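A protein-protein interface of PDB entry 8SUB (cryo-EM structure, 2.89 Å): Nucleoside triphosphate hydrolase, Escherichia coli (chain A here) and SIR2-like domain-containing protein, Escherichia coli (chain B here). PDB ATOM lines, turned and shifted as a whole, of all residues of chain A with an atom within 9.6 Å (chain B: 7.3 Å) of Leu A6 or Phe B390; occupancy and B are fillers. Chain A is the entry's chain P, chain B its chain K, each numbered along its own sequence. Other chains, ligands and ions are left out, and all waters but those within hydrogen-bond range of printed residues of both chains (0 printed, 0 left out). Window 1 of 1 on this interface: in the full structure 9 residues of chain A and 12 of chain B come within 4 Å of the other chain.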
ATOM      1  N   LEU A   3       1.070  13.105  26.638  1.00  0.00           N
ATOM      2  CA  LEU A   3       1.295  14.506  26.310  1.00  0.00           C
ATOM      3  C   LEU A   3       0.338  14.932  25.201  1.00  0.00           C
ATOM      4  O   LEU A   3      -0.375  15.925  25.331  1.00  0.00           O
ATOM      5  CB  LEU A   3       2.750  14.733  25.886  1.00  0.00           C
ATOM      6  CG  LEU A   3       3.308  16.160  25.941  1.00  0.00           C
ATOM      7  CD1 LEU A   3       4.817  16.120  26.129  1.00  0.00           C
ATOM      8  CD2 LEU A   3       2.940  16.983  24.713  1.00  0.00           C
ATOM      9  N   PHE A   4       0.331  14.170  24.112  1.00  0.00           N
ATOM     10  CA  PHE A   4      -0.521  14.437  22.963  1.00  0.00           C
ATOM     11  C   PHE A   4      -1.863  13.750  23.166  1.00  0.00           C
ATOM     12  O   PHE A   4      -1.913  12.563  23.502  1.00  0.00           O
ATOM     13  CB  PHE A   4       0.144  13.950  21.671  1.00  0.00           C
ATOM     14  CG  PHE A   4      -0.564  14.375  20.415  1.00  0.00           C
ATOM     15  CD1 PHE A   4      -0.350  15.626  19.870  1.00  0.00           C
ATOM     16  CD2 PHE A   4      -1.432  13.513  19.771  1.00  0.00           C
ATOM     17  CE1 PHE A   4      -0.997  16.008  18.716  1.00  0.00           C
ATOM     18  CE2 PHE A   4      -2.083  13.897  18.618  1.00  0.00           C
ATOM     19  CZ  PHE A   4      -1.861  15.146  18.090  1.00  0.00           C
ATOM     20  N   LYS A   5      -2.945  14.498  22.968  1.00  0.00           N
ATOM     21  CA  LYS A   5      -4.297  13.988  23.121  1.00  0.00           C
ATOM     22  C   LYS A   5      -5.123  14.379  21.907  1.00  0.00           C
ATOM     23  O   LYS A   5      -4.849  15.387  21.253  1.00  0.00           O
ATOM     24  CB  LYS A   5      -4.967  14.532  24.388  1.00  0.00           C
ATOM     25  CG  LYS A   5      -4.588  13.820  25.670  1.00  0.00           C
ATOM     26  CD  LYS A   5      -5.003  14.647  26.878  1.00  0.00           C
ATOM     27  CE  LYS A   5      -4.067  14.431  28.054  1.00  0.00           C
ATOM     28  NZ  LYS A   5      -4.193  13.061  28.620  1.00  0.00           N
ATOM     29  N   LEU A   6      -6.146  13.579  21.615  1.00  0.00           N
ATOM     30  CA  LEU A   6      -7.043  13.850  20.500  1.00  0.00           C
ATOM     31  C   LEU A   6      -8.338  14.525  20.923  1.00  0.00           C
ATOM     32  O   LEU A   6      -8.868  15.348  20.175  1.00  0.00           O
ATOM     33  CB  LEU A   6      -7.378  12.557  19.749  1.00  0.00           C
ATOM     34  CG  LEU A   6      -6.286  11.887  18.914  1.00  0.00           C
ATOM     35  CD1 LEU A   6      -6.894  10.797  18.060  1.00  0.00           C
ATOM     36  CD2 LEU A   6      -5.558  12.886  18.048  1.00  0.00           C
ATOM     37  N   THR A   7      -8.867  14.197  22.101  1.00  0.00           N
ATOM     38  CA  THR A   7     -10.139  14.741  22.556  1.00  0.00           C
ATOM     39  C   THR A   7     -10.064  14.988  24.057  1.00  0.00           C
ATOM     40  O   THR A   7      -9.081  14.643  24.717  1.00  0.00           O
ATOM     41  CB  THR A   7     -11.302  13.805  22.212  1.00  0.00           C
ATOM     42  OG1 THR A   7     -12.543  14.456  22.500  1.00  0.00           O
ATOM     43  CG2 THR A   7     -11.211  12.529  23.030  1.00  0.00           C
ATOM     44  N   GLU A   8     -11.120  15.596  24.599  1.00  0.00           N
ATOM     45  CA  GLU A   8     -11.148  15.978  26.006  1.00  0.00           C
ATOM     46  C   GLU A   8     -12.383  15.459  26.743  1.00  0.00           C
ATOM     47  O   GLU A   8     -12.296  15.107  27.922  1.00  0.00           O
ATOM     48  CB  GLU A   8     -11.063  17.499  26.126  1.00  0.00           C
ATOM     49  CG  GLU A   8     -11.851  18.234  25.055  1.00  0.00           C
ATOM     50  CD  GLU A   8     -11.614  19.730  25.065  1.00  0.00           C
ATOM     51  OE1 GLU A   8     -10.893  20.219  25.961  1.00  0.00           O
ATOM     52  OE2 GLU A   8     -12.162  20.421  24.182  1.00  0.00           O
ATOM     53  N   ILE A   9     -13.532  15.410  26.073  1.00  0.00           N
ATOM     54  CA  ILE A   9     -14.765  14.925  26.682  1.00  0.00           C
ATOM     55  C   ILE A   9     -14.984  13.479  26.251  1.00  0.00           C
ATOM     56  O   ILE A   9     -14.710  13.092  25.113  1.00  0.00           O
ATOM     57  CB  ILE A   9     -15.992  15.806  26.324  1.00  0.00           C
ATOM     58  CG1 ILE A   9     -15.845  17.226  26.871  1.00  0.00           C
ATOM     59  CG2 ILE A   9     -17.276  15.219  26.869  1.00  0.00           C
ATOM     60  CD1 ILE A   9     -15.183  18.191  25.938  1.00  0.00           C
ATOM     61  N   ASP A  55     -20.339  13.645  17.462  1.00  0.00           N
ATOM     62  CA  ASP A  55     -19.062  13.971  16.842  1.00  0.00           C
ATOM     63  C   ASP A  55     -19.063  13.524  15.385  1.00  0.00           C
ATOM     64  O   ASP A  55     -19.147  12.327  15.100  1.00  0.00           O
ATOM     65  CB  ASP A  55     -17.928  13.303  17.614  1.00  0.00           C
ATOM     66  CG  ASP A  55     -16.565  13.645  17.061  1.00  0.00           C
ATOM     67  OD1 ASP A  55     -16.444  14.667  16.355  1.00  0.00           O
ATOM     68  OD2 ASP A  55     -15.608  12.892  17.339  1.00  0.00           O
ATOM     69  N   GLY A  57     -16.761  14.804  12.756  1.00  0.00           N
ATOM     70  CA  GLY A  57     -15.625  15.331  12.028  1.00  0.00           C
ATOM     71  C   GLY A  57     -15.375  16.807  12.244  1.00  0.00           C
ATOM     72  O   GLY A  57     -14.864  17.203  13.292  1.00  0.00           O
ATOM     73  N   ASN A  58     -15.723  17.632  11.261  1.00  0.00           N
ATOM     74  CA  ASN A  58     -15.497  19.066  11.346  1.00  0.00           C
ATOM     75  C   ASN A  58     -16.737  19.851  11.762  1.00  0.00           C
ATOM     76  O   ASN A  58     -16.684  21.083  11.791  1.00  0.00           O
ATOM     77  CB  ASN A  58     -14.967  19.600  10.012  1.00  0.00           C
ATOM     78  CG  ASN A  58     -15.915  19.355   8.864  1.00  0.00           C
ATOM     79  OD1 ASN A  58     -16.727  18.437   8.902  1.00  0.00           O
ATOM     80  ND2 ASN A  58     -15.809  20.173   7.829  1.00  0.00           N
ATOM     81  N   LEU A  60     -20.444  19.620  14.559  1.00  0.00           N
ATOM     82  CA  LEU A  60     -21.089  18.987  15.703  1.00  0.00           C
ATOM     83  C   LEU A  60     -22.592  19.104  15.519  1.00  0.00           C
ATOM     84  O   LEU A  60     -23.106  20.206  15.337  1.00  0.00           O
ATOM     85  CB  LEU A  60     -20.644  19.646  17.013  1.00  0.00           C
ATOM     86  CG  LEU A  60     -21.170  19.114  18.346  1.00  0.00           C
ATOM     87  CD1 LEU A  60     -20.307  17.993  18.862  1.00  0.00           C
ATOM     88  CD2 LEU A  60     -21.242  20.230  19.362  1.00  0.00           C
ATOM     89  N   ARG A 104     -16.865  25.642  12.753  1.00  0.00           N
ATOM     90  CA  ARG A 104     -15.757  26.547  13.023  1.00  0.00           C
ATOM     91  C   ARG A 104     -15.782  27.748  12.078  1.00  0.00           C
ATOM     92  O   ARG A 104     -16.434  27.741  11.031  1.00  0.00           O
ATOM     93  CB  ARG A 104     -14.422  25.818  12.886  1.00  0.00           C
ATOM     94  CG  ARG A 104     -13.882  25.224  14.173  1.00  0.00           C
ATOM     95  CD  ARG A 104     -12.457  24.747  13.965  1.00  0.00           C
ATOM     96  NE  ARG A 104     -11.945  23.943  15.068  1.00  0.00           N
ATOM     97  CZ  ARG A 104     -11.423  24.442  16.178  1.00  0.00           C
ATOM     98  NH1 ARG A 104     -11.386  25.742  16.398  1.00  0.00           N
ATOM     99  NH2 ARG A 104     -10.939  23.613  17.096  1.00  0.00           N
ATOM    100  N   TYR A 109     -16.683  30.089  16.690  1.00  0.00           N
ATOM    101  CA  TYR A 109     -17.706  29.158  16.246  1.00  0.00           C
ATOM    102  C   TYR A 109     -18.972  29.928  15.909  1.00  0.00           C
ATOM    103  O   TYR A 109     -19.132  31.090  16.284  1.00  0.00           O
ATOM    104  CB  TYR A 109     -18.017  28.106  17.312  1.00  0.00           C
ATOM    105  CG  TYR A 109     -16.822  27.364  17.870  1.00  0.00           C
ATOM    106  CD1 TYR A 109     -16.066  27.898  18.900  1.00  0.00           C
ATOM    107  CD2 TYR A 109     -16.475  26.109  17.389  1.00  0.00           C
ATOM    108  CE1 TYR A 109     -14.990  27.218  19.417  1.00  0.00           C
ATOM    109  CE2 TYR A 109     -15.399  25.424  17.903  1.00  0.00           C
ATOM    110  CZ  TYR A 109     -14.665  25.982  18.917  1.00  0.00           C
ATOM    111  OH  TYR A 109     -13.591  25.303  19.432  1.00  0.00           O
ATOM    112  N   PHE A 132     -20.334  25.398  24.724  1.00  0.00           N
ATOM    113  CA  PHE A 132     -21.210  25.192  23.582  1.00  0.00           C
ATOM    114  C   PHE A 132     -22.613  25.714  23.850  1.00  0.00           C
ATOM    115  O   PHE A 132     -23.283  26.170  22.920  1.00  0.00           O
ATOM    116  CB  PHE A 132     -21.225  23.715  23.200  1.00  0.00           C
ATOM    117  CG  PHE A 132     -19.947  23.253  22.567  1.00  0.00           C
ATOM    118  CD1 PHE A 132     -19.550  23.756  21.344  1.00  0.00           C
ATOM    119  CD2 PHE A 132     -19.133  22.339  23.201  1.00  0.00           C
ATOM    120  CE1 PHE A 132     -18.374  23.348  20.757  1.00  0.00           C
ATOM    121  CE2 PHE A 132     -17.952  21.926  22.614  1.00  0.00           C
ATOM    122  CZ  PHE A 132     -17.575  22.435  21.393  1.00  0.00           C
ATOM    123  N   SER B 149       0.235  18.201  13.698  1.00  0.00           N
ATOM    124  CA  SER B 149      -0.932  17.944  14.532  1.00  0.00           C
ATOM    125  C   SER B 149      -2.182  17.755  13.681  1.00  0.00           C
ATOM    126  O   SER B 149      -3.027  16.909  13.983  1.00  0.00           O
ATOM    127  CB  SER B 149      -1.113  19.087  15.519  1.00  0.00           C
ATOM    128  OG  SER B 149       0.133  19.394  16.105  1.00  0.00           O
ATOM    129  N   LYS B 150      -2.309  18.519  12.596  1.00  0.00           N
ATOM    130  CA  LYS B 150      -3.500  18.418  11.762  1.00  0.00           C
ATOM    131  C   LYS B 150      -3.525  17.124  10.962  1.00  0.00           C
ATOM    132  O   LYS B 150      -4.597  16.568  10.719  1.00  0.00           O
ATOM    133  CB  LYS B 150      -3.578  19.607  10.818  1.00  0.00           C
ATOM    134  CG  LYS B 150      -4.174  20.862  11.463  1.00  0.00           C
ATOM    135  CD  LYS B 150      -4.203  21.947  10.389  1.00  0.00           C
ATOM    136  CE  LYS B 150      -4.851  23.198  10.876  1.00  0.00           C
ATOM    137  NZ  LYS B 150      -5.019  24.351   9.975  1.00  0.00           N
ATOM    138  N   ILE B 152      -2.241  14.082  11.751  1.00  0.00           N
ATOM    139  CA  ILE B 152      -2.458  12.891  12.569  1.00  0.00           C
ATOM    140  C   ILE B 152      -3.905  12.812  13.060  1.00  0.00           C
ATOM    141  O   ILE B 152      -4.535  11.752  13.003  1.00  0.00           O
ATOM    142  CB  ILE B 152      -1.445  12.895  13.730  1.00  0.00           C
ATOM    143  CG1 ILE B 152      -0.080  12.417  13.235  1.00  0.00           C
ATOM    144  CG2 ILE B 152      -1.889  11.989  14.863  1.00  0.00           C
ATOM    145  CD1 ILE B 152       0.991  12.454  14.271  1.00  0.00           C
ATOM    146  N   SER B 153      -4.462  13.922  13.540  1.00  0.00           N
ATOM    147  CA  SER B 153      -5.753  13.855  14.218  1.00  0.00           C
ATOM    148  C   SER B 153      -6.940  13.741  13.272  1.00  0.00           C
ATOM    149  O   SER B 153      -8.075  13.763  13.749  1.00  0.00           O
ATOM    150  CB  SER B 153      -5.959  15.069  15.124  1.00  0.00           C
ATOM    151  OG  SER B 153      -5.953  16.281  14.398  1.00  0.00           O
ATOM    152  N   ASN B 154      -6.726  13.631  11.963  1.00  0.00           N
ATOM    153  CA  ASN B 154      -7.813  13.464  11.005  1.00  0.00           C
ATOM    154  C   ASN B 154      -7.969  12.025  10.533  1.00  0.00           C
ATOM    155  O   ASN B 154      -8.696  11.780   9.566  1.00  0.00           O
ATOM    156  CB  ASN B 154      -7.604  14.378   9.795  1.00  0.00           C
ATOM    157  CG  ASN B 154      -8.075  15.798  10.039  1.00  0.00           C
ATOM    158  OD1 ASN B 154      -9.239  16.038  10.341  1.00  0.00           O
ATOM    159  ND2 ASN B 154      -7.166  16.749   9.902  1.00  0.00           N
ATOM    160  N   ARG B 155      -7.308  11.074  11.179  1.00  0.00           N
ATOM    161  CA  ARG B 155      -7.388   9.671  10.800  1.00  0.00           C
ATOM    162  C   ARG B 155      -8.276   8.914  11.777  1.00  0.00           C
ATOM    163  O   ARG B 155      -8.257   9.177  12.982  1.00  0.00           O
ATOM    164  CB  ARG B 155      -6.003   9.023  10.757  1.00  0.00           C
ATOM    165  CG  ARG B 155      -4.963   9.749   9.926  1.00  0.00           C
ATOM    166  CD  ARG B 155      -5.318   9.784   8.455  1.00  0.00           C
ATOM    167  NE  ARG B 155      -5.047   8.520   7.785  1.00  0.00           N
ATOM    168  CZ  ARG B 155      -5.449   8.229   6.557  1.00  0.00           C
ATOM    169  NH1 ARG B 155      -6.118   9.099   5.825  1.00  0.00           N
ATOM    170  NH2 ARG B 155      -5.172   7.035   6.052  1.00  0.00           N
ATOM    171  N   LEU B 180       6.223  17.805  20.432  1.00  0.00           N
ATOM    172  CA  LEU B 180       4.826  17.419  20.566  1.00  0.00           C
ATOM    173  C   LEU B 180       4.631  16.076  21.250  1.00  0.00           C
ATOM    174  O   LEU B 180       3.550  15.827  21.789  1.00  0.00           O
ATOM    175  CB  LEU B 180       4.159  17.336  19.197  1.00  0.00           C
ATOM    176  CG  LEU B 180       3.690  18.580  18.464  1.00  0.00           C
ATOM    177  CD1 LEU B 180       3.443  18.205  17.021  1.00  0.00           C
ATOM    178  CD2 LEU B 180       2.439  19.119  19.088  1.00  0.00           C
ATOM    179  N   TYR B 219       1.378   7.430  18.900  1.00  0.00           N
ATOM    180  CA  TYR B 219       1.094   8.086  17.632  1.00  0.00           C
ATOM    181  C   TYR B 219       2.405   8.304  16.893  1.00  0.00           C
ATOM    182  O   TYR B 219       3.393   8.729  17.497  1.00  0.00           O
ATOM    183  CB  TYR B 219       0.373   9.414  17.856  1.00  0.00           C
ATOM    184  CG  TYR B 219      -0.992   9.271  18.490  1.00  0.00           C
ATOM    185  CD1 TYR B 219      -2.059   8.754  17.773  1.00  0.00           C
ATOM    186  CD2 TYR B 219      -1.210   9.652  19.804  1.00  0.00           C
ATOM    187  CE1 TYR B 219      -3.301   8.623  18.346  1.00  0.00           C
ATOM    188  CE2 TYR B 219      -2.452   9.524  20.387  1.00  0.00           C
ATOM    189  CZ  TYR B 219      -3.490   9.006  19.653  1.00  0.00           C
ATOM    190  OH  TYR B 219      -4.728   8.877  20.230  1.00  0.00           O
ATOM    191  N   TYR B 386      -9.040  21.487  11.633  1.00  0.00           N
ATOM    192  CA  TYR B 386      -9.143  20.823  12.927  1.00  0.00           C
ATOM    193  C   TYR B 386     -10.478  20.082  13.042  1.00  0.00           C
ATOM    194  O   TYR B 386     -11.472  20.472  12.422  1.00  0.00           O
ATOM    195  CB  TYR B 386      -9.081  21.814  14.075  1.00  0.00           C
ATOM    196  CG  TYR B 386      -7.794  22.551  14.400  1.00  0.00           C
ATOM    197  CD1 TYR B 386      -6.584  22.150  13.909  1.00  0.00           C
ATOM    198  CD2 TYR B 386      -7.836  23.693  15.177  1.00  0.00           C
ATOM    199  CE1 TYR B 386      -5.441  22.846  14.244  1.00  0.00           C
ATOM    200  CE2 TYR B 386      -6.686  24.384  15.471  1.00  0.00           C
ATOM    201  CZ  TYR B 386      -5.498  23.968  14.988  1.00  0.00           C
ATOM    202  OH  TYR B 386      -4.343  24.634  15.305  1.00  0.00           O
ATOM    203  N   PRO B 387     -10.535  19.019  13.839  1.00  0.00           N
ATOM    204  CA  PRO B 387     -11.832  18.559  14.349  1.00  0.00           C
ATOM    205  C   PRO B 387     -12.395  19.544  15.363  1.00  0.00           C
ATOM    206  O   PRO B 387     -11.670  20.335  15.966  1.00  0.00           O
ATOM    207  CB  PRO B 387     -11.498  17.220  15.004  1.00  0.00           C
ATOM    208  CG  PRO B 387     -10.269  16.783  14.323  1.00  0.00           C
ATOM    209  CD  PRO B 387      -9.480  18.019  14.042  1.00  0.00           C
ATOM    210  N   VAL B 388     -13.714  19.493  15.543  1.00  0.00           N
ATOM    211  CA  VAL B 388     -14.380  20.498  16.365  1.00  0.00           C
ATOM    212  C   VAL B 388     -14.087  20.298  17.850  1.00  0.00           C
ATOM    213  O   VAL B 388     -14.144  21.254  18.632  1.00  0.00           O
ATOM    214  CB  VAL B 388     -15.889  20.490  16.064  1.00  0.00           C
ATOM    215  CG1 VAL B 388     -16.536  19.267  16.664  1.00  0.00           C
ATOM    216  CG2 VAL B 388     -16.538  21.767  16.554  1.00  0.00           C
ATOM    217  N   LEU B 389     -13.771  19.074  18.269  1.00  0.00           N
ATOM    218  CA  LEU B 389     -13.558  18.768  19.677  1.00  0.00           C
ATOM    219  C   LEU B 389     -12.087  18.685  20.060  1.00  0.00           C
ATOM    220  O   LEU B 389     -11.776  18.217  21.156  1.00  0.00           O
ATOM    221  CB  LEU B 389     -14.262  17.465  20.052  1.00  0.00           C
ATOM    222  CG  LEU B 389     -15.794  17.469  20.116  1.00  0.00           C
ATOM    223  CD1 LEU B 389     -16.322  16.082  20.393  1.00  0.00           C
ATOM    224  CD2 LEU B 389     -16.311  18.436  21.160  1.00  0.00           C
ATOM    225  N   PHE B 390     -11.183  19.123  19.192  1.00  0.00           N
ATOM    226  CA  PHE B 390      -9.762  19.124  19.515  1.00  0.00           C
ATOM    227  C   PHE B 390      -9.464  20.137  20.619  1.00  0.00           C
ATOM    228  O   PHE B 390     -10.011  21.243  20.615  1.00  0.00           O
ATOM    229  CB  PHE B 390      -8.944  19.448  18.266  1.00  0.00           C
ATOM    230  CG  PHE B 390      -7.484  19.134  18.392  1.00  0.00           C
ATOM    231  CD1 PHE B 390      -7.041  17.827  18.409  1.00  0.00           C
ATOM    232  CD2 PHE B 390      -6.550  20.147  18.472  1.00  0.00           C
ATOM    233  CE1 PHE B 390      -5.701  17.540  18.522  1.00  0.00           C
ATOM    234  CE2 PHE B 390      -5.210  19.861  18.578  1.00  0.00           C
ATOM    235  CZ  PHE B 390      -4.786  18.558  18.603  1.00  0.00           C
ATOM    236  N   PRO B 391      -8.602  19.793  21.578  1.00  0.00           N
ATOM    237  CA  PRO B 391      -8.296  20.723  22.670  1.00  0.00           C
ATOM    238  C   PRO B 391      -7.248  21.745  22.277  1.00  0.00           C
ATOM    239  O   PRO B 391      -6.195  21.409  21.733  1.00  0.00           O
ATOM    240  CB  PRO B 391      -7.770  19.802  23.774  1.00  0.00           C
ATOM    241  CG  PRO B 391      -7.166  18.675  23.041  1.00  0.00           C
ATOM    242  CD  PRO B 391      -7.976  18.478  21.789  1.00  0.00           C
ATOM    243  N   ARG B 392      -7.530  23.006  22.585  1.00  0.00           N
ATOM    244  CA  ARG B 392      -6.593  24.078  22.289  1.00  0.00           C
ATOM    245  C   ARG B 392      -6.486  25.027  23.471  1.00  0.00           C
ATOM    246  O   ARG B 392      -7.416  25.782  23.750  1.00  0.00           O
ATOM    247  CB  ARG B 392      -7.032  24.847  21.049  1.00  0.00           C
ATOM    248  CG  ARG B 392      -6.738  24.161  19.734  1.00  0.00           C
ATOM    249  CD  ARG B 392      -7.535  24.838  18.648  1.00  0.00           C
ATOM    250  NE  ARG B 392      -6.926  26.105  18.267  1.00  0.00           N
ATOM    251  CZ  ARG B 392      -7.497  27.010  17.483  1.00  0.00           C
ATOM    252  NH1 ARG B 392      -8.729  26.855  17.033  1.00  0.00           N
ATOM    253  NH2 ARG B 392      -6.814  28.100  17.148  1.00  0.00           N
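O of Gly A57 is in hydrogen-bond range of N of Val B388, 3.4 Å away.
The guanidinium group of Arg A104 lies close to the guanidinium group of Arg B392 (2.9 Å).
OG of Ser B153 is in hydrogen-bond range of O of Ser B149 (3.0 Å).
Among the printed residues, merely in contact across the chains: Leu A3 with Leu B180, Gly A57 with Pro B387, Arg A104 with Pro B387, Leu A6 with Phe B390, Lys A5 with Phe B390, Leu A6 with Tyr B219, Leu A6 with Pro B391, Arg A104 with Tyr B386, Leu A6 with Ser B153, Glu A8 with Leu B389, Glu A8 with Pro B391, Phe A4 with Tyr B219 and Phe A4 with Leu B180.
Leu A6 touches four residues of chain B.
Thr A7 touches none of the printed residues of chain B.
Printed residues of chain B within 4 Å of Glu A8: Leu B389 and Pro B391.
Printed residues of chain B within 4 Å of Gly A57: Pro B387 (3.5 Å) and Val B388 (3.4 Å).
Of chain A, only Gly A57 (3.5 Å) and Arg A104 (3.5 Å) come within 4 Å of Pro B387.
Of the printed residues of chain A, Leu B389 touches Glu A8 (3.8 Å).
Phe B390 touches just these residues of chain A: Lys A5 (3.6 Å) and Leu A6 (3.5 Å).
Of chain A, only Leu A6 and Glu A8 come within 4 Å of Pro B391.
The nearest residue of chain B that does not touch Leu A6 is Leu B389 (4.2 Å).
The nearest residue of chain A that does not touch Phe B390 is Glu A8 (4.2 Å).
Hydrophobic or aromatic side chains of chain B within 4 Å of the printed part of chain A: Tyr B219, Tyr B386, Pro B387, Phe B390 and Pro B391.
Printed residues of chain A that touch a printed residue of chain B: Leu A3, Phe A4, Lys A5, Leu A6, Glu A8, Gly A57 and Arg A104.
Among the printed residues, 15 pairs touch across the chains.
Among the printed residues, no Asp or Glu carboxylate lies within 4 Å of a Lys or Arg side-chain nitrogen of the other chain.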
